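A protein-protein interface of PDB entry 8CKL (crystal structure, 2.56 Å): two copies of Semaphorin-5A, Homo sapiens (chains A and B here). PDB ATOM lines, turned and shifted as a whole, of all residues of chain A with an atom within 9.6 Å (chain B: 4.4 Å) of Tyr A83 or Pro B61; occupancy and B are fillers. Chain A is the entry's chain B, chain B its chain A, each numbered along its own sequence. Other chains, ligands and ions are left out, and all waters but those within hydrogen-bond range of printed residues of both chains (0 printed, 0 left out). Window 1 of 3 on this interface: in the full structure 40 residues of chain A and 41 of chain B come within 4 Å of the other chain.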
ATOM      1  N   LYS A  57       0.369  10.613  12.509  1.00  0.00           N
ATOM      2  CA  LYS A  57       0.765  11.958  12.112  1.00  0.00           C
ATOM      3  C   LYS A  57       0.830  12.048  10.595  1.00  0.00           C
ATOM      4  O   LYS A  57       1.508  11.240   9.949  1.00  0.00           O
ATOM      5  CB  LYS A  57       2.133  12.321  12.698  1.00  0.00           C
ATOM      6  CG  LYS A  57       2.215  12.290  14.212  1.00  0.00           C
ATOM      7  CD  LYS A  57       3.665  12.259  14.695  1.00  0.00           C
ATOM      8  CE  LYS A  57       4.376  13.598  14.514  1.00  0.00           C
ATOM      9  NZ  LYS A  57       4.875  13.832  13.127  1.00  0.00           N
ATOM     10  N   LYS A  58       0.122  13.022  10.028  1.00  0.00           N
ATOM     11  CA  LYS A  58       0.173  13.287   8.595  1.00  0.00           C
ATOM     12  C   LYS A  58       0.494  14.755   8.368  1.00  0.00           C
ATOM     13  O   LYS A  58      -0.182  15.631   8.911  1.00  0.00           O
ATOM     14  CB  LYS A  58      -1.141  12.909   7.902  1.00  0.00           C
ATOM     15  CG  LYS A  58      -1.351  11.409   7.789  1.00  0.00           C
ATOM     16  CD  LYS A  58      -2.471  11.070   6.822  1.00  0.00           C
ATOM     17  CE  LYS A  58      -2.554   9.569   6.593  1.00  0.00           C
ATOM     18  NZ  LYS A  58      -3.598   9.217   5.591  1.00  0.00           N
ATOM     19  N   THR A  59       1.521  15.022   7.566  1.00  0.00           N
ATOM     20  CA  THR A  59       1.954  16.388   7.307  1.00  0.00           C
ATOM     21  C   THR A  59       1.164  16.987   6.152  1.00  0.00           C
ATOM     22  O   THR A  59       0.847  16.301   5.177  1.00  0.00           O
ATOM     23  CB  THR A  59       3.448  16.433   6.983  1.00  0.00           C
ATOM     24  OG1 THR A  59       3.672  15.886   5.678  1.00  0.00           O
ATOM     25  CG2 THR A  59       4.241  15.631   8.004  1.00  0.00           C
ATOM     26  N   THR A  60       0.850  18.273   6.269  1.00  0.00           N
ATOM     27  CA  THR A  60       0.155  18.973   5.206  1.00  0.00           C
ATOM     28  C   THR A  60       1.121  19.282   4.067  1.00  0.00           C
ATOM     29  O   THR A  60       2.336  19.347   4.272  1.00  0.00           O
ATOM     30  CB  THR A  60      -0.455  20.269   5.736  1.00  0.00           C
ATOM     31  OG1 THR A  60       0.592  21.148   6.169  1.00  0.00           O
ATOM     32  CG2 THR A  60      -1.383  19.984   6.907  1.00  0.00           C
ATOM     33  N   PRO A  61       0.609  19.463   2.850  1.00  0.00           N
ATOM     34  CA  PRO A  61       1.488  19.867   1.747  1.00  0.00           C
ATOM     35  C   PRO A  61       2.113  21.226   2.019  1.00  0.00           C
ATOM     36  O   PRO A  61       1.521  22.088   2.672  1.00  0.00           O
ATOM     37  CB  PRO A  61       0.544  19.913   0.540  1.00  0.00           C
ATOM     38  CG  PRO A  61      -0.567  18.984   0.899  1.00  0.00           C
ATOM     39  CD  PRO A  61      -0.748  19.134   2.383  1.00  0.00           C
ATOM     40  N   TRP A  62       3.330  21.405   1.515  1.00  0.00           N
ATOM     41  CA  TRP A  62       4.044  22.657   1.716  1.00  0.00           C
ATOM     42  C   TRP A  62       3.336  23.805   1.006  1.00  0.00           C
ATOM     43  O   TRP A  62       2.821  23.647  -0.105  1.00  0.00           O
ATOM     44  CB  TRP A  62       5.479  22.543   1.200  1.00  0.00           C
ATOM     45  CG  TRP A  62       6.408  21.748   2.070  1.00  0.00           C
ATOM     46  CD1 TRP A  62       6.844  20.475   1.850  1.00  0.00           C
ATOM     47  CD2 TRP A  62       7.037  22.183   3.283  1.00  0.00           C
ATOM     48  NE1 TRP A  62       7.697  20.085   2.855  1.00  0.00           N
ATOM     49  CE2 TRP A  62       7.833  21.116   3.747  1.00  0.00           C
ATOM     50  CE3 TRP A  62       7.000  23.367   4.026  1.00  0.00           C
ATOM     51  CZ2 TRP A  62       8.585  21.198   4.918  1.00  0.00           C
ATOM     52  CZ3 TRP A  62       7.749  23.447   5.188  1.00  0.00           C
ATOM     53  CH2 TRP A  62       8.528  22.368   5.623  1.00  0.00           C
ATOM     54  N   THR A  63       3.310  24.964   1.657  1.00  0.00           N
ATOM     55  CA  THR A  63       2.819  26.167   1.007  1.00  0.00           C
ATOM     56  C   THR A  63       3.796  26.589  -0.091  1.00  0.00           C
ATOM     57  O   THR A  63       4.987  26.276  -0.023  1.00  0.00           O
ATOM     58  CB  THR A  63       2.645  27.298   2.017  1.00  0.00           C
ATOM     59  OG1 THR A  63       3.872  27.501   2.729  1.00  0.00           O
ATOM     60  CG2 THR A  63       1.537  26.963   3.003  1.00  0.00           C
ATOM     61  N   ARG A  80       8.498  28.818   3.313  1.00  0.00           N
ATOM     62  CA  ARG A  80       7.218  28.149   3.149  1.00  0.00           C
ATOM     63  C   ARG A  80       6.859  27.451   4.452  1.00  0.00           C
ATOM     64  O   ARG A  80       7.727  27.130   5.267  1.00  0.00           O
ATOM     65  CB  ARG A  80       7.242  27.161   1.980  1.00  0.00           C
ATOM     66  CG  ARG A  80       8.211  26.009   2.137  1.00  0.00           C
ATOM     67  CD  ARG A  80       8.043  25.027   0.993  1.00  0.00           C
ATOM     68  NE  ARG A  80       8.884  23.848   1.141  1.00  0.00           N
ATOM     69  CZ  ARG A  80       8.908  22.836   0.284  1.00  0.00           C
ATOM     70  NH1 ARG A  80       8.146  22.831  -0.798  1.00  0.00           N
ATOM     71  NH2 ARG A  80       9.714  21.806   0.517  1.00  0.00           N
ATOM     72  N   PHE A  81       5.564  27.214   4.637  1.00  0.00           N
ATOM     73  CA  PHE A  81       5.035  26.703   5.890  1.00  0.00           C
ATOM     74  C   PHE A  81       4.232  25.431   5.651  1.00  0.00           C
ATOM     75  O   PHE A  81       3.712  25.192   4.557  1.00  0.00           O
ATOM     76  CB  PHE A  81       4.143  27.747   6.578  1.00  0.00           C
ATOM     77  CG  PHE A  81       4.775  29.105   6.701  1.00  0.00           C
ATOM     78  CD1 PHE A  81       4.710  30.014   5.657  1.00  0.00           C
ATOM     79  CD2 PHE A  81       5.422  29.480   7.867  1.00  0.00           C
ATOM     80  CE1 PHE A  81       5.285  31.264   5.768  1.00  0.00           C
ATOM     81  CE2 PHE A  81       5.999  30.728   7.985  1.00  0.00           C
ATOM     82  CZ  PHE A  81       5.929  31.622   6.934  1.00  0.00           C
ATOM     83  N   ARG A  82       4.143  24.609   6.694  1.00  0.00           N
ATOM     84  CA  ARG A  82       3.307  23.417   6.659  1.00  0.00           C
ATOM     85  C   ARG A  82       2.951  23.042   8.089  1.00  0.00           C
ATOM     86  O   ARG A  82       3.604  23.471   9.044  1.00  0.00           O
ATOM     87  CB  ARG A  82       3.985  22.249   5.935  1.00  0.00           C
ATOM     88  CG  ARG A  82       4.874  21.379   6.805  1.00  0.00           C
ATOM     89  CD  ARG A  82       5.438  20.236   5.981  1.00  0.00           C
ATOM     90  NE  ARG A  82       6.200  19.282   6.778  1.00  0.00           N
ATOM     91  CZ  ARG A  82       6.709  18.155   6.300  1.00  0.00           C
ATOM     92  NH1 ARG A  82       6.565  17.815   5.031  1.00  0.00           N
ATOM     93  NH2 ARG A  82       7.379  17.348   7.118  1.00  0.00           N
ATOM     94  N   TYR A  83       1.905  22.231   8.222  1.00  0.00           N
ATOM     95  CA  TYR A  83       1.404  21.803   9.518  1.00  0.00           C
ATOM     96  C   TYR A  83       1.310  20.285   9.546  1.00  0.00           C
ATOM     97  O   TYR A  83       1.472  19.609   8.526  1.00  0.00           O
ATOM     98  CB  TYR A  83       0.033  22.425   9.818  1.00  0.00           C
ATOM     99  CG  TYR A  83       0.063  23.928   9.965  1.00  0.00           C
ATOM    100  CD1 TYR A  83      -0.174  24.755   8.876  1.00  0.00           C
ATOM    101  CD2 TYR A  83       0.338  24.518  11.190  1.00  0.00           C
ATOM    102  CE1 TYR A  83      -0.144  26.129   9.003  1.00  0.00           C
ATOM    103  CE2 TYR A  83       0.369  25.894  11.328  1.00  0.00           C
ATOM    104  CZ  TYR A  83       0.129  26.694  10.230  1.00  0.00           C
ATOM    105  OH  TYR A  83       0.159  28.062  10.359  1.00  0.00           O
ATOM    106  N   THR A  84       1.049  19.749  10.735  1.00  0.00           N
ATOM    107  CA  THR A  84       0.901  18.316  10.931  1.00  0.00           C
ATOM    108  C   THR A  84      -0.393  18.037  11.679  1.00  0.00           C
ATOM    109  O   THR A  84      -0.726  18.733  12.642  1.00  0.00           O
ATOM    110  CB  THR A  84       2.083  17.727  11.714  1.00  0.00           C
ATOM    111  OG1 THR A  84       2.290  18.486  12.910  1.00  0.00           O
ATOM    112  CG2 THR A  84       3.351  17.762  10.874  1.00  0.00           C
ATOM    113  N   CYS A  85      -1.116  17.016  11.230  1.00  0.00           N
ATOM    114  CA  CYS A  85      -2.339  16.565  11.875  1.00  0.00           C
ATOM    115  C   CYS A  85      -2.043  15.288  12.646  1.00  0.00           C
ATOM    116  O   CYS A  85      -1.484  14.337  12.088  1.00  0.00           O
ATOM    117  CB  CYS A  85      -3.439  16.315  10.843  1.00  0.00           C
ATOM    118  SG  CYS A  85      -3.766  17.696   9.720  1.00  0.00           S
ATOM    119  N   LYS A  86      -2.420  15.270  13.922  1.00  0.00           N
ATOM    120  CA  LYS A  86      -2.181  14.139  14.806  1.00  0.00           C
ATOM    121  C   LYS A  86      -3.518  13.623  15.314  1.00  0.00           C
ATOM    122  O   LYS A  86      -4.364  14.411  15.748  1.00  0.00           O
ATOM    123  CB  LYS A  86      -1.282  14.536  15.980  1.00  0.00           C
ATOM    124  CG  LYS A  86       0.030  15.182  15.566  1.00  0.00           C
ATOM    125  CD  LYS A  86       0.633  15.987  16.705  1.00  0.00           C
ATOM    126  CE  LYS A  86       1.029  15.088  17.865  1.00  0.00           C
ATOM    127  NZ  LYS A  86       1.650  15.857  18.978  1.00  0.00           N
ATOM    128  N   VAL A  97      -5.650  14.916   5.110  1.00  0.00           N
ATOM    129  CA  VAL A  97      -5.401  16.352   5.108  1.00  0.00           C
ATOM    130  C   VAL A  97      -6.293  16.982   4.049  1.00  0.00           C
ATOM    131  O   VAL A  97      -6.365  16.492   2.915  1.00  0.00           O
ATOM    132  CB  VAL A  97      -3.919  16.666   4.848  1.00  0.00           C
ATOM    133  CG1 VAL A  97      -3.706  18.169   4.747  1.00  0.00           C
ATOM    134  CG2 VAL A  97      -3.054  16.074   5.947  1.00  0.00           C
ATOM    135  N   GLY A  98      -6.970  18.064   4.417  1.00  0.00           N
ATOM    136  CA  GLY A  98      -7.946  18.684   3.552  1.00  0.00           C
ATOM    137  C   GLY A  98      -7.341  19.573   2.483  1.00  0.00           C
ATOM    138  O   GLY A  98      -6.131  19.601   2.245  1.00  0.00           O
ATOM    139  N   GLN A 100      -6.310  23.025   0.368  1.00  0.00           N
ATOM    140  CA  GLN A 100      -5.589  24.248   0.695  1.00  0.00           C
ATOM    141  C   GLN A 100      -6.520  25.444   0.543  1.00  0.00           C
ATOM    142  O   GLN A 100      -7.084  25.665  -0.535  1.00  0.00           O
ATOM    143  CB  GLN A 100      -4.364  24.403  -0.204  1.00  0.00           C
ATOM    144  CG  GLN A 100      -3.418  25.512   0.228  1.00  0.00           C
ATOM    145  CD  GLN A 100      -2.257  25.695  -0.728  1.00  0.00           C
ATOM    146  OE1 GLN A 100      -1.163  26.087  -0.326  1.00  0.00           O
ATOM    147  NE2 GLN A 100      -2.491  25.413  -2.005  1.00  0.00           N
ATOM    148  N   ARG A 101      -6.680  26.214   1.615  1.00  0.00           N
ATOM    149  CA  ARG A 101      -7.518  27.404   1.615  1.00  0.00           C
ATOM    150  C   ARG A 101      -6.621  28.631   1.619  1.00  0.00           C
ATOM    151  O   ARG A 101      -5.706  28.734   2.444  1.00  0.00           O
ATOM    152  CB  ARG A 101      -8.454  27.420   2.826  1.00  0.00           C
ATOM    153  CG  ARG A 101      -9.428  26.255   2.865  1.00  0.00           C
ATOM    154  CD  ARG A 101     -10.160  26.187   4.193  1.00  0.00           C
ATOM    155  NE  ARG A 101     -11.106  25.079   4.236  1.00  0.00           N
ATOM    156  CZ  ARG A 101     -11.967  24.868   5.222  1.00  0.00           C
ATOM    157  NH1 ARG A 101     -12.029  25.672   6.270  1.00  0.00           N
ATOM    158  NH2 ARG A 101     -12.784  23.820   5.155  1.00  0.00           N
ATOM    159  N   GLU A 103      -6.321  32.962   1.397  1.00  0.00           N
ATOM    160  CA  GLU A 103      -6.927  34.277   1.554  1.00  0.00           C
ATOM    161  C   GLU A 103      -6.037  35.298   0.863  1.00  0.00           C
ATOM    162  O   GLU A 103      -4.814  35.278   1.030  1.00  0.00           O
ATOM    163  CB  GLU A 103      -7.105  34.645   3.030  1.00  0.00           C
ATOM    164  CG  GLU A 103      -8.493  34.364   3.581  1.00  0.00           C
ATOM    165  CD  GLU A 103      -8.672  34.876   4.998  1.00  0.00           C
ATOM    166  OE1 GLU A 103      -7.678  35.339   5.596  1.00  0.00           O
ATOM    167  OE2 GLU A 103      -9.809  34.817   5.512  1.00  0.00           O
ATOM    168  N   THR B  59      -9.439  23.238  11.429  1.00  0.00           N
ATOM    169  CA  THR B  59      -8.632  24.077  10.555  1.00  0.00           C
ATOM    170  C   THR B  59      -7.339  24.491  11.248  1.00  0.00           C
ATOM    171  O   THR B  59      -7.312  24.728  12.460  1.00  0.00           O
ATOM    172  CB  THR B  59      -9.418  25.312  10.104  1.00  0.00           C
ATOM    173  OG1 THR B  59      -8.676  26.006   9.093  1.00  0.00           O
ATOM    174  CG2 THR B  59      -9.679  26.256  11.266  1.00  0.00           C
ATOM    175  N   THR B  60      -6.262  24.538  10.473  1.00  0.00           N
ATOM    176  CA  THR B  60      -4.963  24.963  10.966  1.00  0.00           C
ATOM    177  C   THR B  60      -4.907  26.481  11.104  1.00  0.00           C
ATOM    178  O   THR B  60      -5.683  27.201  10.470  1.00  0.00           O
ATOM    179  CB  THR B  60      -3.862  24.484  10.024  1.00  0.00           C
ATOM    180  OG1 THR B  60      -4.024  25.104   8.742  1.00  0.00           O
ATOM    181  CG2 THR B  60      -3.917  22.971   9.865  1.00  0.00           C
ATOM    182  N   PRO B  61      -4.007  26.994  11.943  1.00  0.00           N
ATOM    183  CA  PRO B  61      -3.831  28.447  12.031  1.00  0.00           C
ATOM    184  C   PRO B  61      -3.382  29.030  10.700  1.00  0.00           C
ATOM    185  O   PRO B  61      -2.718  28.370   9.898  1.00  0.00           O
ATOM    186  CB  PRO B  61      -2.751  28.611  13.107  1.00  0.00           C
ATOM    187  CG  PRO B  61      -2.856  27.375  13.931  1.00  0.00           C
ATOM    188  CD  PRO B  61      -3.224  26.283  12.969  1.00  0.00           C
ATOM    189  N   TRP B  62      -3.773  30.280  10.464  1.00  0.00           N
ATOM    190  CA  TRP B  62      -3.433  30.946   9.214  1.00  0.00           C
ATOM    191  C   TRP B  62      -1.928  31.139   9.077  1.00  0.00           C
ATOM    192  O   TRP B  62      -1.227  31.432  10.049  1.00  0.00           O
ATOM    193  CB  TRP B  62      -4.133  32.303   9.124  1.00  0.00           C
ATOM    194  CG  TRP B  62      -5.591  32.220   8.804  1.00  0.00           C
ATOM    195  CD1 TRP B  62      -6.631  32.386   9.670  1.00  0.00           C
ATOM    196  CD2 TRP B  62      -6.173  31.951   7.523  1.00  0.00           C
ATOM    197  NE1 TRP B  62      -7.826  32.238   9.006  1.00  0.00           N
ATOM    198  CE2 TRP B  62      -7.571  31.970   7.687  1.00  0.00           C
ATOM    199  CE3 TRP B  62      -5.646  31.696   6.253  1.00  0.00           C
ATOM    200  CZ2 TRP B  62      -8.449  31.744   6.630  1.00  0.00           C
ATOM    201  CZ3 TRP B  62      -6.520  31.471   5.206  1.00  0.00           C
ATOM    202  CH2 TRP B  62      -7.904  31.494   5.401  1.00  0.00           C
ATOM    203  N   THR B  63      -1.439  30.964   7.853  1.00  0.00           N
ATOM    204  CA  THR B  63      -0.055  31.262   7.535  1.00  0.00           C
ATOM    205  C   THR B  63       0.178  32.772   7.626  1.00  0.00           C
ATOM    206  O   THR B  63      -0.740  33.560   7.383  1.00  0.00           O
ATOM    207  CB  THR B  63       0.261  30.745   6.126  1.00  0.00           C
ATOM    208  OG1 THR B  63       0.392  29.317   6.156  1.00  0.00           O
ATOM    209  CG2 THR B  63       1.520  31.364   5.530  1.00  0.00           C
ATOM    210  N   PHE B  81      -2.156  31.063   3.710  1.00  0.00           N
ATOM    211  CA  PHE B  81      -2.662  29.720   3.481  1.00  0.00           C
ATOM    212  C   PHE B  81      -3.059  29.050   4.790  1.00  0.00           C
ATOM    213  O   PHE B  81      -2.584  29.408   5.871  1.00  0.00           O
ATOM    214  CB  PHE B  81      -1.613  28.862   2.759  1.00  0.00           C
ATOM    215  CG  PHE B  81      -1.037  29.512   1.532  1.00  0.00           C
ATOM    216  CD1 PHE B  81      -1.561  29.242   0.281  1.00  0.00           C
ATOM    217  CD2 PHE B  81       0.030  30.390   1.629  1.00  0.00           C
ATOM    218  CE1 PHE B  81      -1.039  29.838  -0.851  1.00  0.00           C
ATOM    219  CE2 PHE B  81       0.559  30.990   0.500  1.00  0.00           C
ATOM    220  CZ  PHE B  81       0.023  30.713  -0.742  1.00  0.00           C
ATOM    221  N   ARG B  82      -3.948  28.067   4.674  1.00  0.00           N
ATOM    222  CA  ARG B  82      -4.355  27.258   5.812  1.00  0.00           C
ATOM    223  C   ARG B  82      -4.828  25.905   5.301  1.00  0.00           C
ATOM    224  O   ARG B  82      -5.200  25.755   4.134  1.00  0.00           O
ATOM    225  CB  ARG B  82      -5.466  27.939   6.620  1.00  0.00           C
ATOM    226  CG  ARG B  82      -6.863  27.635   6.104  1.00  0.00           C
ATOM    227  CD  ARG B  82      -7.936  28.323   6.927  1.00  0.00           C
ATOM    228  NE  ARG B  82      -7.576  28.443   8.334  1.00  0.00           N
ATOM    229  CZ  ARG B  82      -8.348  29.002   9.255  1.00  0.00           C
ATOM    230  NH1 ARG B  82      -9.539  29.492   8.954  1.00  0.00           N
ATOM    231  NH2 ARG B  82      -7.915  29.071  10.510  1.00  0.00           N
ATOM    232  N   VAL B  97      -3.907  19.587  15.893  1.00  0.00           N
ATOM    233  CA  VAL B  97      -3.039  20.159  14.870  1.00  0.00           C
ATOM    234  C   VAL B  97      -1.696  20.469  15.514  1.00  0.00           C
ATOM    235  O   VAL B  97      -1.645  21.057  16.600  1.00  0.00           O
ATOM    236  CB  VAL B  97      -3.659  21.421  14.247  1.00  0.00           C
ATOM    237  CG1 VAL B  97      -2.695  22.056  13.256  1.00  0.00           C
ATOM    238  CG2 VAL B  97      -4.980  21.086  13.574  1.00  0.00           C
ATOM    239  N   GLY B  98      -0.614  20.074  14.850  1.00  0.00           N
ATOM    240  CA  GLY B  98       0.710  20.222  15.410  1.00  0.00           C
ATOM    241  C   GLY B  98       1.245  21.635  15.269  1.00  0.00           C
ATOM    242  O   GLY B  98       0.544  22.573  14.888  1.00  0.00           O
ATOM    243  N   ARG B  99       2.528  21.775  15.590  1.00  0.00           N
ATOM    244  CA  ARG B  99       3.180  23.074  15.560  1.00  0.00           C
ATOM    245  C   ARG B  99       3.448  23.510  14.122  1.00  0.00           C
ATOM    246  O   ARG B  99       3.513  22.697  13.197  1.00  0.00           O
ATOM    247  CB  ARG B  99       4.488  23.037  16.350  1.00  0.00           C
ATOM    248  N   GLN B 100       3.605  24.820  13.943  1.00  0.00           N
ATOM    249  CA  GLN B 100       3.903  25.376  12.629  1.00  0.00           C
ATOM    250  C   GLN B 100       5.384  25.193  12.326  1.00  0.00           C
ATOM    251  O   GLN B 100       6.243  25.670  13.074  1.00  0.00           O
ATOM    252  CB  GLN B 100       3.525  26.852  12.567  1.00  0.00           C
ATOM    253  CG  GLN B 100       3.588  27.444  11.167  1.00  0.00           C
ATOM    254  CD  GLN B 100       3.290  28.930  11.144  1.00  0.00           C
ATOM    255  OE1 GLN B 100       2.148  29.349  11.332  1.00  0.00           O
ATOM    256  NE2 GLN B 100       4.321  29.737  10.915  1.00  0.00           N
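Of chain B, only Thr B60, Pro B61, Trp B62 and Gln B100 come within 4 Å of Tyr A83.
Printed residues of chain A within 4 Å of Pro B61: Tyr A83 (2.9 Å).
Thr B60 touches one residue of chain A.
Printed residues of chain A within 4 Å of Thr B63: Phe A81.
Of the printed residues of chain A, Phe B81 touches Thr A63, Gln A100 and Arg A101.
The nearest printed residue of chain B that does not touch Tyr A83 is Thr B63 (4.2 Å).
Thr A63 touches Phe B81, and with the chains exchanged Phe A81 touches Thr B63.
Phe A81 touches Gln B100, and with the chains exchanged Gln A100 touches Phe B81.
Gln A100 touches Arg B82, but with the chains exchanged Arg A82 does not touch Gln B100 (4.1 Å).
10 positions are printed for both chains.
The backbone carbonyl oxygen (O) of Arg A101 sits at hydrogen-bond distance from the backbone NH (N) of Arg B82 (2.9 Å).
The backbone NH of Gly B98 is in hydrogen-bond range of the backbone carbonyl oxygen of Thr A84 (2.6 Å).
The side-chain amide oxygen (OE1) of Gln B100 is in hydrogen-bond range of the side-chain hydroxyl (OH) of Tyr A83 (2.6 Å).
The side-chain hydroxyl of Tyr A83 lies within hydrogen-bond range of the backbone carbonyl oxygen of Pro B61 (2.9 Å).
Of the 11 printed residues of chain B, 9 touch a printed residue of chain A.
Hydrophobic or aromatic side chains of chain B that line the printed part of chain A: Pro B61, Trp B62, Phe B81 and Val B97.
Among the printed residues, no Asp or Glu carboxylate lies within 4 Å of a Lys or Arg side-chain nitrogen of the other chain.
CG2 of Thr A63 touches CB of Phe B81, 3.7 Å away.
Gln B100 touches Phe A81.
Tyr A83 touches Thr B60 (CD1 to OG1, 3.9 Å).
O of Trp B62 touches OH of Tyr A83, 3.7 Å away.
O of Thr A84 touches C of Val B97 (3.5 Å).
Phe B81 touches Gln A100 (CD1 to OE1, 3.2 Å).
Gln A100 touches Arg B82.
Trp B62 touches Arg A101.
O of Arg A101 touches CA of Phe B81 (3.4 Å).
Glu A103 touches Trp B62 (CG to CH2, 3.4 Å).
The backbone NH (N) of Thr B63 sits at hydrogen-bond distance from the backbone carbonyl oxygen (O) of Phe B81.
OG1 of Thr B59 lies within hydrogen-bond range of NE of Arg B82 (2.8 Å).
The backbone NH of Tyr A83 sits at hydrogen-bond distance from the side-chain hydroxyl of Thr A60, at 2.7 Å.
The backbone carbonyl oxygen of Thr B60 sits at hydrogen-bond distance from the guanidinium group of Arg B82, 2.9 Å away.
The side-chain hydroxyl (OG1) of Thr A63 is in hydrogen-bond range of the backbone NH (N) of Phe A81 (2.6 Å).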
